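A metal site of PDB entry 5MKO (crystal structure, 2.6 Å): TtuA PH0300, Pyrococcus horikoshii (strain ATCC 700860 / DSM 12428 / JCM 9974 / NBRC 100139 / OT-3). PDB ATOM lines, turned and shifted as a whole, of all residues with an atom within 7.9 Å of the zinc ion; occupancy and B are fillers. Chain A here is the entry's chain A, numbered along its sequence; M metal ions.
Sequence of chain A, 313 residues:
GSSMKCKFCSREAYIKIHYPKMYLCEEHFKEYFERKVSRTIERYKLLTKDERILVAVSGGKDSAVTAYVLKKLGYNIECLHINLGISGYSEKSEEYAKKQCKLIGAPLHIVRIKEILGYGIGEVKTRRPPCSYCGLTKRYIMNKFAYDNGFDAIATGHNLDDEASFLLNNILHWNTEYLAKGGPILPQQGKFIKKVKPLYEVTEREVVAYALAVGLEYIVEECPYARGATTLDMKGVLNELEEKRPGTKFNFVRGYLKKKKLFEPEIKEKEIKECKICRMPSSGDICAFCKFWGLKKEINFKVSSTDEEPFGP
The zinc ion is bound by SG of Cys 287, SG of Cys 275, SG of Cys 278 and SG of Cys 290.
Of the 21 residues printed, 4 come within 4 Å of the zinc ion. Along chain A the residues within 4 Å of the zinc ion span positions 275 to 290.
OG of Ser 282 sits at hydrogen-bond distance from N of Cys 287, 3.2 Å away. The backbone NH of Ile 277 sits close to the side-chain sulfur of Cys 275 (3.4 Å). The backbone NH (N) of Cys 275 sits at hydrogen-bond distance from the backbone carbonyl oxygen (O) of Met 280, at 3.0 Å. OH of Tyr 140 sits close to SG of Cys 278 (3.0 Å). The side-chain sulfur of Cys 278 sits close to the backbone NH of Met 280. The backbone carbonyl oxygen of Cys 290 lies within hydrogen-bond range of the backbone NH of Leu 295 (2.9 Å).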
ATOM      1  N   TYR A 140      -9.077 -14.541  -6.368  1.00  0.00           N
ATOM      2  CA  TYR A 140      -9.592 -13.642  -5.330  1.00  0.00           C
ATOM      3  C   TYR A 140      -9.201 -12.195  -5.601  1.00  0.00           C
ATOM      4  O   TYR A 140     -10.060 -11.323  -5.560  1.00  0.00           O
ATOM      5  CB  TYR A 140      -9.095 -14.071  -3.927  1.00  0.00           C
ATOM      6  CG  TYR A 140      -9.493 -13.106  -2.835  1.00  0.00           C
ATOM      7  CD1 TYR A 140      -8.730 -11.965  -2.575  1.00  0.00           C
ATOM      8  CD2 TYR A 140     -10.649 -13.306  -2.084  1.00  0.00           C
ATOM      9  CE1 TYR A 140      -9.112 -11.039  -1.601  1.00  0.00           C
ATOM     10  CE2 TYR A 140     -11.030 -12.398  -1.087  1.00  0.00           C
ATOM     11  CZ  TYR A 140     -10.250 -11.272  -0.851  1.00  0.00           C
ATOM     12  OH  TYR A 140     -10.613 -10.368   0.121  1.00  0.00           O
ATOM     13  N   LYS A 144     -11.739  -9.204  -6.299  1.00  0.00           N
ATOM     14  CA  LYS A 144     -11.833  -8.059  -5.398  1.00  0.00           C
ATOM     15  C   LYS A 144     -11.341  -6.778  -6.041  1.00  0.00           C
ATOM     16  O   LYS A 144     -11.923  -5.731  -5.786  1.00  0.00           O
ATOM     17  CB  LYS A 144     -11.172  -8.301  -4.032  1.00  0.00           C
ATOM     18  CG  LYS A 144     -11.810  -7.434  -2.959  1.00  0.00           C
ATOM     19  CD  LYS A 144     -11.220  -7.583  -1.574  1.00  0.00           C
ATOM     20  CE  LYS A 144     -12.100  -6.946  -0.528  1.00  0.00           C
ATOM     21  NZ  LYS A 144     -12.028  -5.461  -0.550  1.00  0.00           N
ATOM     22  N   GLU A 274     -20.877 -14.360   3.954  1.00  0.00           N
ATOM     23  CA  GLU A 274     -19.998 -13.224   3.703  1.00  0.00           C
ATOM     24  C   GLU A 274     -18.847 -13.271   4.717  1.00  0.00           C
ATOM     25  O   GLU A 274     -19.100 -13.473   5.904  1.00  0.00           O
ATOM     26  CB  GLU A 274     -20.757 -11.887   3.804  1.00  0.00           C
ATOM     27  CG  GLU A 274     -21.835 -11.690   2.757  1.00  0.00           C
ATOM     28  CD  GLU A 274     -21.395 -11.013   1.478  1.00  0.00           C
ATOM     29  OE1 GLU A 274     -21.681  -9.798   1.319  1.00  0.00           O
ATOM     30  OE2 GLU A 274     -20.759 -11.685   0.629  1.00  0.00           O
ATOM     31  N   CYS A 275     -17.599 -13.109   4.236  1.00  0.00           N
ATOM     32  CA  CYS A 275     -16.398 -13.163   5.077  1.00  0.00           C
ATOM     33  C   CYS A 275     -16.362 -12.067   6.166  1.00  0.00           C
ATOM     34  O   CYS A 275     -16.536 -10.896   5.858  1.00  0.00           O
ATOM     35  CB  CYS A 275     -15.130 -13.136   4.223  1.00  0.00           C
ATOM     36  SG  CYS A 275     -13.591 -13.090   5.170  1.00  0.00           S
ATOM     37  N   LYS A 276     -16.129 -12.487   7.414  1.00  0.00           N
ATOM     38  CA  LYS A 276     -16.048 -11.644   8.619  1.00  0.00           C
ATOM     39  C   LYS A 276     -14.948 -10.561   8.512  1.00  0.00           C
ATOM     40  O   LYS A 276     -15.023  -9.551   9.221  1.00  0.00           O
ATOM     41  CB  LYS A 276     -15.789 -12.534   9.840  1.00  0.00           C
ATOM     42  CG  LYS A 276     -16.414 -12.051  11.137  1.00  0.00           C
ATOM     43  CD  LYS A 276     -16.648 -13.231  12.081  1.00  0.00           C
ATOM     44  CE  LYS A 276     -15.980 -13.060  13.418  1.00  0.00           C
ATOM     45  NZ  LYS A 276     -16.248 -14.218  14.316  1.00  0.00           N
ATOM     46  N   ILE A 277     -13.948 -10.781   7.634  1.00  0.00           N
ATOM     47  CA  ILE A 277     -12.782  -9.915   7.445  1.00  0.00           C
ATOM     48  C   ILE A 277     -12.900  -8.973   6.235  1.00  0.00           C
ATOM     49  O   ILE A 277     -12.670  -7.773   6.392  1.00  0.00           O
ATOM     50  CB  ILE A 277     -11.458 -10.752   7.400  1.00  0.00           C
ATOM     51  CG1 ILE A 277     -11.359 -11.805   8.562  1.00  0.00           C
ATOM     52  CG2 ILE A 277     -10.198  -9.884   7.307  1.00  0.00           C
ATOM     53  CD1 ILE A 277     -11.309 -11.266  10.053  1.00  0.00           C
ATOM     54  N   CYS A 278     -13.230  -9.516   5.052  1.00  0.00           N
ATOM     55  CA  CYS A 278     -13.277  -8.759   3.790  1.00  0.00           C
ATOM     56  C   CYS A 278     -14.654  -8.661   3.129  1.00  0.00           C
ATOM     57  O   CYS A 278     -14.753  -8.048   2.054  1.00  0.00           O
ATOM     58  CB  CYS A 278     -12.258  -9.330   2.828  1.00  0.00           C
ATOM     59  SG  CYS A 278     -12.708 -10.969   2.206  1.00  0.00           S
ATOM     60  N   ARG A 279     -15.708  -9.268   3.722  1.00  0.00           N
ATOM     61  CA  ARG A 279     -17.094  -9.281   3.228  1.00  0.00           C
ATOM     62  C   ARG A 279     -17.265  -9.969   1.849  1.00  0.00           C
ATOM     63  O   ARG A 279     -18.369  -9.965   1.290  1.00  0.00           O
ATOM     64  CB  ARG A 279     -17.723  -7.879   3.198  1.00  0.00           C
ATOM     65  CG  ARG A 279     -17.505  -7.012   4.447  1.00  0.00           C
ATOM     66  CD  ARG A 279     -18.642  -6.031   4.647  1.00  0.00           C
ATOM     67  NE  ARG A 279     -19.934  -6.616   4.297  1.00  0.00           N
ATOM     68  CZ  ARG A 279     -20.881  -5.984   3.600  1.00  0.00           C
ATOM     69  NH1 ARG A 279     -21.995  -6.612   3.273  1.00  0.00           N
ATOM     70  NH2 ARG A 279     -20.713  -4.723   3.230  1.00  0.00           N
ATOM     71  N   MET A 280     -16.199 -10.566   1.288  1.00  0.00           N
ATOM     72  CA  MET A 280     -16.268 -11.244  -0.015  1.00  0.00           C
ATOM     73  C   MET A 280     -16.934 -12.617   0.154  1.00  0.00           C
ATOM     74  O   MET A 280     -16.937 -13.132   1.279  1.00  0.00           O
ATOM     75  CB  MET A 280     -14.883 -11.336  -0.699  1.00  0.00           C
ATOM     76  CG  MET A 280     -14.309  -9.984  -1.130  1.00  0.00           C
ATOM     77  SD  MET A 280     -15.440  -8.850  -2.006  1.00  0.00           S
ATOM     78  CE  MET A 280     -15.238  -9.415  -3.673  1.00  0.00           C
ATOM     79  N   PRO A 281     -17.547 -13.226  -0.917  1.00  0.00           N
ATOM     80  CA  PRO A 281     -18.198 -14.540  -0.739  1.00  0.00           C
ATOM     81  C   PRO A 281     -17.325 -15.576  -0.036  1.00  0.00           C
ATOM     82  O   PRO A 281     -16.142 -15.753  -0.388  1.00  0.00           O
ATOM     83  CB  PRO A 281     -18.601 -14.944  -2.152  1.00  0.00           C
ATOM     84  CG  PRO A 281     -18.679 -13.690  -2.913  1.00  0.00           C
ATOM     85  CD  PRO A 281     -17.653 -12.772  -2.328  1.00  0.00           C
ATOM     86  N   SER A 282     -17.898 -16.207   1.001  1.00  0.00           N
ATOM     87  CA  SER A 282     -17.227 -17.144   1.890  1.00  0.00           C
ATOM     88  C   SER A 282     -18.086 -18.369   2.232  1.00  0.00           C
ATOM     89  O   SER A 282     -19.310 -18.323   2.116  1.00  0.00           O
ATOM     90  CB  SER A 282     -16.839 -16.420   3.180  1.00  0.00           C
ATOM     91  OG  SER A 282     -16.367 -17.281   4.205  1.00  0.00           O
ATOM     92  N   ASP A 285     -17.308 -18.516   8.598  1.00  0.00           N
ATOM     93  CA  ASP A 285     -17.028 -17.179   9.172  1.00  0.00           C
ATOM     94  C   ASP A 285     -16.019 -16.376   8.352  1.00  0.00           C
ATOM     95  O   ASP A 285     -16.298 -15.223   7.999  1.00  0.00           O
ATOM     96  CB  ASP A 285     -16.547 -17.299  10.634  1.00  0.00           C
ATOM     97  CG  ASP A 285     -17.604 -17.743  11.624  1.00  0.00           C
ATOM     98  OD1 ASP A 285     -18.024 -18.921  11.560  1.00  0.00           O
ATOM     99  OD2 ASP A 285     -17.973 -16.925  12.497  1.00  0.00           O
ATOM    100  N   ILE A 286     -14.858 -16.991   8.058  1.00  0.00           N
ATOM    101  CA  ILE A 286     -13.751 -16.410   7.305  1.00  0.00           C
ATOM    102  C   ILE A 286     -13.581 -17.184   5.988  1.00  0.00           C
ATOM    103  O   ILE A 286     -13.702 -18.410   5.998  1.00  0.00           O
ATOM    104  CB  ILE A 286     -12.462 -16.423   8.183  1.00  0.00           C
ATOM    105  CG1 ILE A 286     -12.674 -15.633   9.505  1.00  0.00           C
ATOM    106  CG2 ILE A 286     -11.239 -15.890   7.420  1.00  0.00           C
ATOM    107  CD1 ILE A 286     -11.802 -16.077  10.688  1.00  0.00           C
ATOM    108  N   CYS A 287     -13.303 -16.485   4.874  1.00  0.00           N
ATOM    109  CA  CYS A 287     -13.070 -17.124   3.576  1.00  0.00           C
ATOM    110  C   CYS A 287     -11.690 -17.788   3.522  1.00  0.00           C
ATOM    111  O   CYS A 287     -10.820 -17.472   4.339  1.00  0.00           O
ATOM    112  CB  CYS A 287     -13.278 -16.157   2.417  1.00  0.00           C
ATOM    113  SG  CYS A 287     -12.037 -14.843   2.293  1.00  0.00           S
ATOM    114  N   ALA A 288     -11.506 -18.706   2.564  1.00  0.00           N
ATOM    115  CA  ALA A 288     -10.251 -19.441   2.358  1.00  0.00           C
ATOM    116  C   ALA A 288      -9.022 -18.530   2.218  1.00  0.00           C
ATOM    117  O   ALA A 288      -7.960 -18.866   2.722  1.00  0.00           O
ATOM    118  CB  ALA A 288     -10.380 -20.349   1.144  1.00  0.00           C
ATOM    119  N   PHE A 289      -9.199 -17.348   1.557  1.00  0.00           N
ATOM    120  CA  PHE A 289      -8.146 -16.366   1.338  1.00  0.00           C
ATOM    121  C   PHE A 289      -7.618 -15.763   2.646  1.00  0.00           C
ATOM    122  O   PHE A 289      -6.409 -15.809   2.895  1.00  0.00           O
ATOM    123  CB  PHE A 289      -8.616 -15.260   0.363  1.00  0.00           C
ATOM    124  CG  PHE A 289      -7.520 -14.339  -0.121  1.00  0.00           C
ATOM    125  CD1 PHE A 289      -6.758 -14.670  -1.239  1.00  0.00           C
ATOM    126  CD2 PHE A 289      -7.233 -13.151   0.534  1.00  0.00           C
ATOM    127  CE1 PHE A 289      -5.734 -13.829  -1.697  1.00  0.00           C
ATOM    128  CE2 PHE A 289      -6.222 -12.307   0.082  1.00  0.00           C
ATOM    129  CZ  PHE A 289      -5.474 -12.646  -1.029  1.00  0.00           C
ATOM    130  N   CYS A 290      -8.519 -15.205   3.481  1.00  0.00           N
ATOM    131  CA  CYS A 290      -8.152 -14.571   4.741  1.00  0.00           C
ATOM    132  C   CYS A 290      -7.624 -15.571   5.768  1.00  0.00           C
ATOM    133  O   CYS A 290      -6.760 -15.214   6.590  1.00  0.00           O
ATOM    134  CB  CYS A 290      -9.292 -13.732   5.295  1.00  0.00           C
ATOM    135  SG  CYS A 290      -9.585 -12.182   4.397  1.00  0.00           S
ATOM    136  N   LYS A 291      -8.111 -16.820   5.719  1.00  0.00           N
ATOM    137  CA  LYS A 291      -7.690 -17.914   6.592  1.00  0.00           C
ATOM    138  C   LYS A 291      -6.243 -18.299   6.267  1.00  0.00           C
ATOM    139  O   LYS A 291      -5.406 -18.298   7.158  1.00  0.00           O
ATOM    140  CB  LYS A 291      -8.624 -19.126   6.429  1.00  0.00           C
ATOM    141  CG  LYS A 291      -9.662 -19.263   7.532  1.00  0.00           C
ATOM    142  CD  LYS A 291     -10.692 -20.340   7.174  1.00  0.00           C
ATOM    143  CE  LYS A 291     -11.843 -20.387   8.144  1.00  0.00           C
ATOM    144  NZ  LYS A 291     -12.939 -21.270   7.648  1.00  0.00           N
ATOM    145  N   LEU A 295      -5.048 -13.027   7.545  1.00  0.00           N
ATOM    146  CA  LEU A 295      -5.447 -11.618   7.497  1.00  0.00           C
ATOM    147  C   LEU A 295      -6.519 -11.279   8.529  1.00  0.00           C
ATOM    148  O   LEU A 295      -7.511 -11.981   8.644  1.00  0.00           O
ATOM    149  CB  LEU A 295      -5.936 -11.252   6.081  1.00  0.00           C
ATOM    150  CG  LEU A 295      -4.970 -11.502   4.930  1.00  0.00           C
ATOM    151  CD1 LEU A 295      -5.722 -11.698   3.641  1.00  0.00           C
ATOM    152  CD2 LEU A 295      -3.952 -10.369   4.800  1.00  0.00           C
ATOM    153  N   LYS A 297      -7.498  -7.790   8.758  1.00  0.00           N
ATOM    154  CA  LYS A 297      -8.146  -6.640   8.121  1.00  0.00           C
ATOM    155  C   LYS A 297      -8.392  -6.869   6.627  1.00  0.00           C
ATOM    156  O   LYS A 297      -7.798  -7.785   6.022  1.00  0.00           O
ATOM    157  CB  LYS A 297      -7.328  -5.357   8.364  1.00  0.00           C
ATOM    158  CG  LYS A 297      -7.040  -5.035   9.831  1.00  0.00           C
ATOM    159  CD  LYS A 297      -8.256  -4.477  10.590  1.00  0.00           C
ATOM    160  CE  LYS A 297      -8.018  -4.399  12.086  1.00  0.00           C
ATOM    161  NZ  LYS A 297      -9.253  -4.002  12.812  1.00  0.00           N
ATOM    162  N   GLU A 298      -9.300  -6.065   6.031  1.00  0.00           N
ATOM    163  CA  GLU A 298      -9.658  -6.132   4.610  1.00  0.00           C
ATOM    164  C   GLU A 298      -8.624  -5.405   3.752  1.00  0.00           C
ATOM    165  O   GLU A 298      -8.090  -4.375   4.169  1.00  0.00           O
ATOM    166  CB  GLU A 298     -11.051  -5.533   4.379  1.00  0.00           C
ATOM    167  CG  GLU A 298     -11.517  -5.505   2.932  1.00  0.00           C
ATOM    168  CD  GLU A 298     -12.830  -4.807   2.687  1.00  0.00           C
ATOM    169  OE1 GLU A 298     -13.879  -5.386   3.067  1.00  0.00           O
ATOM    170  OE2 GLU A 298     -12.827  -3.706   2.096  1.00  0.00           O
HETATM  171 ZN    ZN M   1     -12.043 -12.984   3.522  1.00  0.00          ZN
